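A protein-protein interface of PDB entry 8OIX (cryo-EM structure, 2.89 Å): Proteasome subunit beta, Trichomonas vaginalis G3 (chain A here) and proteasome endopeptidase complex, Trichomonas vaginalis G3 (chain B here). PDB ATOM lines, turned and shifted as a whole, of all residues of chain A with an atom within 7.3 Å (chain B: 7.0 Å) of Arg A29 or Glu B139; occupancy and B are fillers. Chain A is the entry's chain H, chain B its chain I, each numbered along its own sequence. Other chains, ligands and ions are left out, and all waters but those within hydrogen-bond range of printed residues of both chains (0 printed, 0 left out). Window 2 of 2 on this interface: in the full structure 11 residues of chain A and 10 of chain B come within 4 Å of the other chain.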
ATOM      1  N   ASP A  17      -6.271  30.667  20.370  1.00  0.00           N
ATOM      2  CA  ASP A  17      -4.824  30.709  20.438  1.00  0.00           C
ATOM      3  C   ASP A  17      -4.399  30.476  21.884  1.00  0.00           C
ATOM      4  O   ASP A  17      -5.227  30.390  22.794  1.00  0.00           O
ATOM      5  CB  ASP A  17      -4.291  32.040  19.909  1.00  0.00           C
ATOM      6  CG  ASP A  17      -4.562  33.189  20.851  1.00  0.00           C
ATOM      7  OD1 ASP A  17      -5.746  33.446  21.146  1.00  0.00           O
ATOM      8  OD2 ASP A  17      -3.595  33.837  21.300  1.00  0.00           O
ATOM      9  N   SER A  18      -3.095  30.362  22.099  1.00  0.00           N
ATOM     10  CA  SER A  18      -2.575  30.089  23.431  1.00  0.00           C
ATOM     11  C   SER A  18      -1.606  31.167  23.899  1.00  0.00           C
ATOM     12  O   SER A  18      -0.736  30.903  24.724  1.00  0.00           O
ATOM     13  CB  SER A  18      -1.902  28.720  23.470  1.00  0.00           C
ATOM     14  OG  SER A  18      -0.681  28.734  22.755  1.00  0.00           O
ATOM     15  N   ARG A  19      -1.758  32.389  23.410  1.00  0.00           N
ATOM     16  CA  ARG A  19      -0.798  33.450  23.692  1.00  0.00           C
ATOM     17  C   ARG A  19      -1.428  34.495  24.601  1.00  0.00           C
ATOM     18  O   ARG A  19      -2.330  35.227  24.183  1.00  0.00           O
ATOM     19  CB  ARG A  19      -0.305  34.098  22.403  1.00  0.00           C
ATOM     20  CG  ARG A  19       0.569  35.312  22.646  1.00  0.00           C
ATOM     21  CD  ARG A  19       1.200  35.811  21.369  1.00  0.00           C
ATOM     22  NE  ARG A  19       2.138  34.849  20.808  1.00  0.00           N
ATOM     23  CZ  ARG A  19       2.846  35.054  19.708  1.00  0.00           C
ATOM     24  NH1 ARG A  19       2.648  36.116  18.948  1.00  0.00           N
ATOM     25  NH2 ARG A  19       3.750  34.151  19.342  1.00  0.00           N
ATOM     26  N   THR A  20      -0.957  34.553  25.842  1.00  0.00           N
ATOM     27  CA  THR A  20      -1.240  35.674  26.725  1.00  0.00           C
ATOM     28  C   THR A  20      -0.142  36.703  26.502  1.00  0.00           C
ATOM     29  O   THR A  20       1.042  36.360  26.536  1.00  0.00           O
ATOM     30  CB  THR A  20      -1.273  35.236  28.189  1.00  0.00           C
ATOM     31  OG1 THR A  20      -2.336  34.302  28.388  1.00  0.00           O
ATOM     32  CG2 THR A  20      -1.502  36.435  29.092  1.00  0.00           C
ATOM     33  N   PHE A  25       5.518  41.305  25.358  1.00  0.00           N
ATOM     34  CA  PHE A  25       5.971  40.126  26.079  1.00  0.00           C
ATOM     35  C   PHE A  25       4.833  39.130  26.229  1.00  0.00           C
ATOM     36  O   PHE A  25       3.686  39.514  26.470  1.00  0.00           O
ATOM     37  CB  PHE A  25       6.522  40.490  27.457  1.00  0.00           C
ATOM     38  CG  PHE A  25       6.938  39.300  28.267  1.00  0.00           C
ATOM     39  CD1 PHE A  25       8.007  38.517  27.874  1.00  0.00           C
ATOM     40  CD2 PHE A  25       6.258  38.962  29.424  1.00  0.00           C
ATOM     41  CE1 PHE A  25       8.386  37.416  28.615  1.00  0.00           C
ATOM     42  CE2 PHE A  25       6.638  37.867  30.172  1.00  0.00           C
ATOM     43  CZ  PHE A  25       7.702  37.093  29.766  1.00  0.00           C
ATOM     44  N   ILE A  26       5.152  37.853  26.046  1.00  0.00           N
ATOM     45  CA  ILE A  26       4.188  36.765  26.172  1.00  0.00           C
ATOM     46  C   ILE A  26       4.367  36.090  27.527  1.00  0.00           C
ATOM     47  O   ILE A  26       5.180  35.161  27.644  1.00  0.00           O
ATOM     48  CB  ILE A  26       4.353  35.756  25.024  1.00  0.00           C
ATOM     49  CG1 ILE A  26       4.201  36.457  23.678  1.00  0.00           C
ATOM     50  CG2 ILE A  26       3.345  34.633  25.138  1.00  0.00           C
ATOM     51  CD1 ILE A  26       4.753  35.669  22.526  1.00  0.00           C
ATOM     52  N   PRO A  27       3.670  36.532  28.583  1.00  0.00           N
ATOM     53  CA  PRO A  27       3.812  35.846  29.877  1.00  0.00           C
ATOM     54  C   PRO A  27       3.466  34.372  29.813  1.00  0.00           C
ATOM     55  O   PRO A  27       4.171  33.546  30.405  1.00  0.00           O
ATOM     56  CB  PRO A  27       2.846  36.624  30.784  1.00  0.00           C
ATOM     57  CG  PRO A  27       1.908  37.299  29.837  1.00  0.00           C
ATOM     58  CD  PRO A  27       2.789  37.700  28.709  1.00  0.00           C
ATOM     59  N   ASN A  28       2.393  34.018  29.117  1.00  0.00           N
ATOM     60  CA  ASN A  28       1.997  32.630  28.934  1.00  0.00           C
ATOM     61  C   ASN A  28       1.924  32.343  27.442  1.00  0.00           C
ATOM     62  O   ASN A  28       1.163  32.995  26.719  1.00  0.00           O
ATOM     63  CB  ASN A  28       0.652  32.354  29.608  1.00  0.00           C
ATOM     64  CG  ASN A  28       0.306  30.881  29.641  1.00  0.00           C
ATOM     65  OD1 ASN A  28       1.073  30.040  29.178  1.00  0.00           O
ATOM     66  ND2 ASN A  28      -0.852  30.562  30.200  1.00  0.00           N
ATOM     67  N   ARG A  29       2.695  31.356  26.990  1.00  0.00           N
ATOM     68  CA  ARG A  29       2.709  30.965  25.589  1.00  0.00           C
ATOM     69  C   ARG A  29       1.833  29.756  25.318  1.00  0.00           C
ATOM     70  O   ARG A  29       1.574  29.445  24.151  1.00  0.00           O
ATOM     71  CB  ARG A  29       4.135  30.666  25.127  1.00  0.00           C
ATOM     72  CG  ARG A  29       4.914  29.836  26.110  1.00  0.00           C
ATOM     73  CD  ARG A  29       6.309  29.574  25.609  1.00  0.00           C
ATOM     74  NE  ARG A  29       6.346  28.663  24.477  1.00  0.00           N
ATOM     75  CZ  ARG A  29       6.908  27.463  24.518  1.00  0.00           C
ATOM     76  NH1 ARG A  29       7.619  27.070  25.562  1.00  0.00           N
ATOM     77  NH2 ARG A  29       6.800  26.660  23.466  1.00  0.00           N
ATOM     78  N   ALA A  30       1.378  29.071  26.363  1.00  0.00           N
ATOM     79  CA  ALA A  30       0.455  27.955  26.241  1.00  0.00           C
ATOM     80  C   ALA A  30      -0.725  28.257  27.161  1.00  0.00           C
ATOM     81  O   ALA A  30      -0.868  27.683  28.242  1.00  0.00           O
ATOM     82  CB  ALA A  30       1.130  26.634  26.595  1.00  0.00           C
ATOM     83  N   THR A  31      -1.577  29.171  26.712  1.00  0.00           N
ATOM     84  CA  THR A  31      -2.720  29.616  27.489  1.00  0.00           C
ATOM     85  C   THR A  31      -3.939  28.781  27.141  1.00  0.00           C
ATOM     86  O   THR A  31      -4.183  28.474  25.972  1.00  0.00           O
ATOM     87  CB  THR A  31      -3.014  31.095  27.229  1.00  0.00           C
ATOM     88  OG1 THR A  31      -1.803  31.853  27.344  1.00  0.00           O
ATOM     89  CG2 THR A  31      -4.030  31.618  28.231  1.00  0.00           C
ATOM     90  N   ASN A  32      -4.704  28.415  28.160  1.00  0.00           N
ATOM     91  CA  ASN A  32      -5.975  27.735  27.953  1.00  0.00           C
ATOM     92  C   ASN A  32      -7.046  28.816  28.017  1.00  0.00           C
ATOM     93  O   ASN A  32      -7.629  29.082  29.069  1.00  0.00           O
ATOM     94  CB  ASN A  32      -6.197  26.642  28.989  1.00  0.00           C
ATOM     95  CG  ASN A  32      -7.381  25.763  28.657  1.00  0.00           C
ATOM     96  OD1 ASN A  32      -7.607  25.419  27.497  1.00  0.00           O
ATOM     97  ND2 ASN A  32      -8.151  25.399  29.675  1.00  0.00           N
ATOM     98  N   GLY A 172      -1.011  33.762  19.142  1.00  0.00           N
ATOM     99  CA  GLY A 172       0.110  32.902  18.826  1.00  0.00           C
ATOM    100  C   GLY A 172       0.066  31.650  19.664  1.00  0.00           C
ATOM    101  O   GLY A 172      -0.837  31.448  20.481  1.00  0.00           O
ATOM    102  N   GLY A 173       1.060  30.808  19.444  1.00  0.00           N
ATOM    103  CA  GLY A 173       1.197  29.588  20.215  1.00  0.00           C
ATOM    104  C   GLY A 173       0.508  28.423  19.541  1.00  0.00           C
ATOM    105  O   GLY A 173       0.632  28.237  18.331  1.00  0.00           O
ATOM    106  N   VAL A 174      -0.221  27.643  20.327  1.00  0.00           N
ATOM    107  CA  VAL A 174      -0.899  26.460  19.842  1.00  0.00           C
ATOM    108  C   VAL A 174      -2.379  26.770  19.669  1.00  0.00           C
ATOM    109  O   VAL A 174      -2.928  27.693  20.273  1.00  0.00           O
ATOM    110  CB  VAL A 174      -0.690  25.258  20.787  1.00  0.00           C
ATOM    111  CG1 VAL A 174       0.789  25.021  21.018  1.00  0.00           C
ATOM    112  CG2 VAL A 174      -1.401  25.494  22.103  1.00  0.00           C
ATOM    113  N   ASN A 176      -5.708  25.755  20.616  1.00  0.00           N
ATOM    114  CA  ASN A 176      -6.510  25.011  21.580  1.00  0.00           C
ATOM    115  C   ASN A 176      -7.886  24.755  20.981  1.00  0.00           C
ATOM    116  O   ASN A 176      -8.686  25.682  20.840  1.00  0.00           O
ATOM    117  CB  ASN A 176      -6.622  25.786  22.890  1.00  0.00           C
ATOM    118  CG  ASN A 176      -5.273  26.148  23.472  1.00  0.00           C
ATOM    119  OD1 ASN A 176      -4.456  25.277  23.765  1.00  0.00           O
ATOM    120  ND2 ASN A 176      -5.035  27.441  23.649  1.00  0.00           N
ATOM    121  N   PRO A 192       2.519  24.393  16.885  1.00  0.00           N
ATOM    122  CA  PRO A 192       2.971  25.063  15.655  1.00  0.00           C
ATOM    123  C   PRO A 192       3.488  24.115  14.588  1.00  0.00           C
ATOM    124  O   PRO A 192       3.330  24.396  13.393  1.00  0.00           O
ATOM    125  CB  PRO A 192       4.069  25.991  16.181  1.00  0.00           C
ATOM    126  CG  PRO A 192       3.514  26.405  17.496  1.00  0.00           C
ATOM    127  CD  PRO A 192       3.028  25.097  18.076  1.00  0.00           C
ATOM    128  N   GLN B 122       1.174  26.782  34.116  1.00  0.00           N
ATOM    129  CA  GLN B 122       2.261  26.701  33.155  1.00  0.00           C
ATOM    130  C   GLN B 122       3.345  25.795  33.711  1.00  0.00           C
ATOM    131  O   GLN B 122       3.554  25.748  34.929  1.00  0.00           O
ATOM    132  CB  GLN B 122       2.862  28.079  32.844  1.00  0.00           C
ATOM    133  CG  GLN B 122       1.872  29.131  32.410  1.00  0.00           C
ATOM    134  CD  GLN B 122       2.555  30.406  31.983  1.00  0.00           C
ATOM    135  OE1 GLN B 122       3.371  30.405  31.063  1.00  0.00           O
ATOM    136  NE2 GLN B 122       2.236  31.503  32.657  1.00  0.00           N
ATOM    137  N   PRO B 123       4.044  25.060  32.846  1.00  0.00           N
ATOM    138  CA  PRO B 123       5.148  24.220  33.338  1.00  0.00           C
ATOM    139  C   PRO B 123       6.269  25.015  33.982  1.00  0.00           C
ATOM    140  O   PRO B 123       6.755  24.635  35.054  1.00  0.00           O
ATOM    141  CB  PRO B 123       5.617  23.494  32.074  1.00  0.00           C
ATOM    142  CG  PRO B 123       5.164  24.334  30.950  1.00  0.00           C
ATOM    143  CD  PRO B 123       3.908  25.008  31.382  1.00  0.00           C
ATOM    144  N   PHE B 124       6.702  26.101  33.351  1.00  0.00           N
ATOM    145  CA  PHE B 124       7.728  26.978  33.893  1.00  0.00           C
ATOM    146  C   PHE B 124       7.248  28.415  33.772  1.00  0.00           C
ATOM    147  O   PHE B 124       6.666  28.800  32.755  1.00  0.00           O
ATOM    148  CB  PHE B 124       9.072  26.789  33.177  1.00  0.00           C
ATOM    149  CG  PHE B 124       9.003  26.981  31.692  1.00  0.00           C
ATOM    150  CD1 PHE B 124       9.192  28.230  31.131  1.00  0.00           C
ATOM    151  CD2 PHE B 124       8.755  25.909  30.856  1.00  0.00           C
ATOM    152  CE1 PHE B 124       9.131  28.406  29.770  1.00  0.00           C
ATOM    153  CE2 PHE B 124       8.694  26.080  29.494  1.00  0.00           C
ATOM    154  CZ  PHE B 124       8.881  27.329  28.949  1.00  0.00           C
ATOM    155  N   LEU B 132      12.061  38.236  32.196  1.00  0.00           N
ATOM    156  CA  LEU B 132      12.387  37.879  30.828  1.00  0.00           C
ATOM    157  C   LEU B 132      13.748  37.205  30.775  1.00  0.00           C
ATOM    158  O   LEU B 132      13.881  36.118  30.199  1.00  0.00           O
ATOM    159  CB  LEU B 132      12.347  39.124  29.937  1.00  0.00           C
ATOM    160  CG  LEU B 132      10.981  39.631  29.450  1.00  0.00           C
ATOM    161  CD1 LEU B 132       9.997  39.876  30.580  1.00  0.00           C
ATOM    162  CD2 LEU B 132      11.130  40.890  28.630  1.00  0.00           C
ATOM    163  N   ALA B 134      15.084  35.554  33.076  1.00  0.00           N
ATOM    164  CA  ALA B 134      14.901  34.221  33.629  1.00  0.00           C
ATOM    165  C   ALA B 134      14.176  33.317  32.645  1.00  0.00           C
ATOM    166  O   ALA B 134      14.602  32.177  32.415  1.00  0.00           O
ATOM    167  CB  ALA B 134      14.124  34.294  34.940  1.00  0.00           C
ATOM    168  N   ILE B 135      13.120  33.826  32.004  1.00  0.00           N
ATOM    169  CA  ILE B 135      12.291  32.924  31.215  1.00  0.00           C
ATOM    170  C   ILE B 135      13.069  32.412  30.020  1.00  0.00           C
ATOM    171  O   ILE B 135      12.860  31.273  29.583  1.00  0.00           O
ATOM    172  CB  ILE B 135      10.967  33.597  30.805  1.00  0.00           C
ATOM    173  CG1 ILE B 135       9.901  32.539  30.525  1.00  0.00           C
ATOM    174  CG2 ILE B 135      11.150  34.468  29.590  1.00  0.00           C
ATOM    175  CD1 ILE B 135       9.540  31.707  31.727  1.00  0.00           C
ATOM    176  N   SER B 136      14.050  33.184  29.547  1.00  0.00           N
ATOM    177  CA  SER B 136      14.888  32.708  28.457  1.00  0.00           C
ATOM    178  C   SER B 136      15.555  31.401  28.847  1.00  0.00           C
ATOM    179  O   SER B 136      15.423  30.390  28.144  1.00  0.00           O
ATOM    180  CB  SER B 136      15.931  33.765  28.098  1.00  0.00           C
ATOM    181  OG  SER B 136      16.986  33.775  29.042  1.00  0.00           O
ATOM    182  N   VAL B 137      16.175  31.369  30.029  1.00  0.00           N
ATOM    183  CA  VAL B 137      16.793  30.131  30.482  1.00  0.00           C
ATOM    184  C   VAL B 137      15.722  29.067  30.621  1.00  0.00           C
ATOM    185  O   VAL B 137      15.865  27.942  30.121  1.00  0.00           O
ATOM    186  CB  VAL B 137      17.547  30.360  31.805  1.00  0.00           C
ATOM    187  CG1 VAL B 137      18.109  29.051  32.330  1.00  0.00           C
ATOM    188  CG2 VAL B 137      18.645  31.388  31.620  1.00  0.00           C
ATOM    189  N   LEU B 138      14.585  29.448  31.201  1.00  0.00           N
ATOM    190  CA  LEU B 138      13.497  28.503  31.386  1.00  0.00           C
ATOM    191  C   LEU B 138      12.989  28.021  30.041  1.00  0.00           C
ATOM    192  O   LEU B 138      12.610  26.855  29.892  1.00  0.00           O
ATOM    193  CB  LEU B 138      12.382  29.155  32.202  1.00  0.00           C
ATOM    194  CG  LEU B 138      12.160  28.636  33.621  1.00  0.00           C
ATOM    195  CD1 LEU B 138      13.469  28.525  34.361  1.00  0.00           C
ATOM    196  CD2 LEU B 138      11.221  29.567  34.363  1.00  0.00           C
ATOM    197  N   GLU B 139      12.969  28.909  29.046  1.00  0.00           N
ATOM    198  CA  GLU B 139      12.498  28.508  27.731  1.00  0.00           C
ATOM    199  C   GLU B 139      13.453  27.513  27.091  1.00  0.00           C
ATOM    200  O   GLU B 139      13.025  26.612  26.361  1.00  0.00           O
ATOM    201  CB  GLU B 139      12.315  29.735  26.842  1.00  0.00           C
ATOM    202  CG  GLU B 139      11.069  30.502  27.191  1.00  0.00           C
ATOM    203  CD  GLU B 139       9.804  29.801  26.773  1.00  0.00           C
ATOM    204  OE1 GLU B 139       9.875  28.736  26.126  1.00  0.00           O
ATOM    205  OE2 GLU B 139       8.730  30.294  27.155  1.00  0.00           O
ATOM    206  N   ASN B 140      14.751  27.663  27.349  1.00  0.00           N
ATOM    207  CA  ASN B 140      15.746  26.870  26.643  1.00  0.00           C
ATOM    208  C   ASN B 140      16.134  25.591  27.366  1.00  0.00           C
ATOM    209  O   ASN B 140      16.637  24.665  26.721  1.00  0.00           O
ATOM    210  CB  ASN B 140      16.995  27.714  26.393  1.00  0.00           C
ATOM    211  CG  ASN B 140      16.711  28.912  25.518  1.00  0.00           C
ATOM    212  OD1 ASN B 140      16.994  30.049  25.891  1.00  0.00           O
ATOM    213  ND2 ASN B 140      16.132  28.666  24.352  1.00  0.00           N
ATOM    214  N   ARG B 141      15.914  25.511  28.673  1.00  0.00           N
ATOM    215  CA  ARG B 141      16.405  24.388  29.452  1.00  0.00           C
ATOM    216  C   ARG B 141      15.312  23.562  30.117  1.00  0.00           C
ATOM    217  O   ARG B 141      15.631  22.552  30.752  1.00  0.00           O
ATOM    218  CB  ARG B 141      17.389  24.885  30.517  1.00  0.00           C
ATOM    219  CG  ARG B 141      18.670  25.450  29.935  1.00  0.00           C
ATOM    220  CD  ARG B 141      19.581  25.974  31.023  1.00  0.00           C
ATOM    221  NE  ARG B 141      19.850  24.962  32.036  1.00  0.00           N
ATOM    222  CZ  ARG B 141      20.614  25.160  33.100  1.00  0.00           C
ATOM    223  NH1 ARG B 141      21.271  26.291  33.275  1.00  0.00           N
ATOM    224  NH2 ARG B 141      20.744  24.186  33.995  1.00  0.00           N
ATOM    225  N   TRP B 142      14.045  23.944  29.993  1.00  0.00           N
ATOM    226  CA  TRP B 142      12.967  23.149  30.564  1.00  0.00           C
ATOM    227  C   TRP B 142      12.470  22.138  29.543  1.00  0.00           C
ATOM    228  O   TRP B 142      12.261  22.474  28.373  1.00  0.00           O
ATOM    229  CB  TRP B 142      11.802  24.020  31.038  1.00  0.00           C
ATOM    230  CG  TRP B 142      10.762  23.201  31.744  1.00  0.00           C
ATOM    231  CD1 TRP B 142      10.694  22.947  33.081  1.00  0.00           C
ATOM    232  CD2 TRP B 142       9.674  22.487  31.144  1.00  0.00           C
ATOM    233  NE1 TRP B 142       9.623  22.137  33.355  1.00  0.00           N
ATOM    234  CE2 TRP B 142       8.980  21.839  32.182  1.00  0.00           C
ATOM    235  CE3 TRP B 142       9.214  22.341  29.832  1.00  0.00           C
ATOM    236  CZ2 TRP B 142       7.857  21.053  31.950  1.00  0.00           C
ATOM    237  CZ3 TRP B 142       8.097  21.565  29.606  1.00  0.00           C
ATOM    238  CH2 TRP B 142       7.429  20.932  30.658  1.00  0.00           C
ATOM    239  N   HIS B 143      12.283  20.900  29.993  1.00  0.00           N
ATOM    240  CA  HIS B 143      11.705  19.856  29.167  1.00  0.00           C
ATOM    241  C   HIS B 143      10.863  18.956  30.057  1.00  0.00           C
ATOM    242  O   HIS B 143      11.032  18.927  31.278  1.00  0.00           O
ATOM    243  CB  HIS B 143      12.784  19.051  28.437  1.00  0.00           C
ATOM    244  CG  HIS B 143      13.759  18.379  29.352  1.00  0.00           C
ATOM    245  ND1 HIS B 143      14.915  18.991  29.784  1.00  0.00           N
ATOM    246  CD2 HIS B 143      13.754  17.146  29.910  1.00  0.00           C
ATOM    247  CE1 HIS B 143      15.579  18.165  30.573  1.00  0.00           C
ATOM    248  NE2 HIS B 143      14.896  17.038  30.664  1.00  0.00           N
ATOM    249  N   MET B 154      18.501  24.687  36.413  1.00  0.00           N
ATOM    250  CA  MET B 154      17.858  25.564  35.441  1.00  0.00           C
ATOM    251  C   MET B 154      17.186  26.747  36.120  1.00  0.00           C
ATOM    252  O   MET B 154      17.301  27.884  35.653  1.00  0.00           O
ATOM    253  CB  MET B 154      16.837  24.788  34.622  1.00  0.00           C
ATOM    254  CG  MET B 154      16.044  25.676  33.696  1.00  0.00           C
ATOM    255  SD  MET B 154      14.574  24.852  33.101  1.00  0.00           S
ATOM    256  CE  MET B 154      13.702  24.628  34.638  1.00  0.00           C
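OE1 of Gln B122 lies close to OD1 of Asn A28, at 3.0 Å.
The guanidinium group (NH1) of Arg A29 is in salt-bridge range of the side-chain carboxylate (OE1) of Glu B139 (2.9 Å).
The backbone carbonyl oxygen (O) of Pro A27 lies close to the side-chain amide oxygen (OE1) of Gln B122 (3.3 Å).
OG1 of Thr A31 sits at hydrogen-bond distance from O of Asn A28, 3.2 Å away.
OD1 of Asn A28 sits at hydrogen-bond distance from N of Ala A30 (3.0 Å).
The side-chain hydroxyl (OG) of Ser A18 lies within hydrogen-bond range of the backbone carbonyl oxygen (O) of Arg A29 (2.7 Å).
O of Asn A28 lies within hydrogen-bond range of N of Thr A20 (2.8 Å).
Among the printed residues, merely in contact across the chains: Phe A25 with Leu B132 and Arg A29 with Phe B124.
Arg A29 touches just these residues of chain B: Phe B124 (3.6 Å) and Glu B139 (2.9 Å).
Printed residues of chain A within 4 Å of Phe B124: Arg A29.
Of the printed residues of chain B, Pro A27 touches Gln B122 (3.3 Å).
Printed residues of chain A within 4 Å of Gln B122: Pro A27 and Asn A28.
Of the printed residues of chain B, Phe A25 touches Leu B132 (3.5 Å).
Asn A32 touches none of the printed residues of chain B.
The nearest residue of chain B that does not touch Arg A29 is Gln B122 (4.2 Å).
The nearest residue of chain A that does not touch Glu B139 is Ile A26 (6.0 Å).
The nearest printed residue of chain B that does not touch Pro A27 is Ile B135 (5.8 Å).
Of the 17 printed residues of chain A, 4 touch a printed residue of chain B.
Hydrophobic or aromatic side chains of chain A that line the printed part of chain B: Phe A25.
Printed residues of chain B that touch a printed residue of chain A: Gln B122, Phe B124, Leu B132 and Glu B139.
Hydrophobic or aromatic side chains of chain B within 4 Å of the printed part of chain A: Phe B124 and Leu B132.
Along chain B the printed residues that touch a printed residue of chain A span positions 122 to 139.
Among the printed residues, 5 pairs touch across the chains.
Among the printed residues, Asp or Glu carboxylates within 4 Å of a Lys or Arg side-chain nitrogen of the other chain: Arg A29 with Glu B139.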
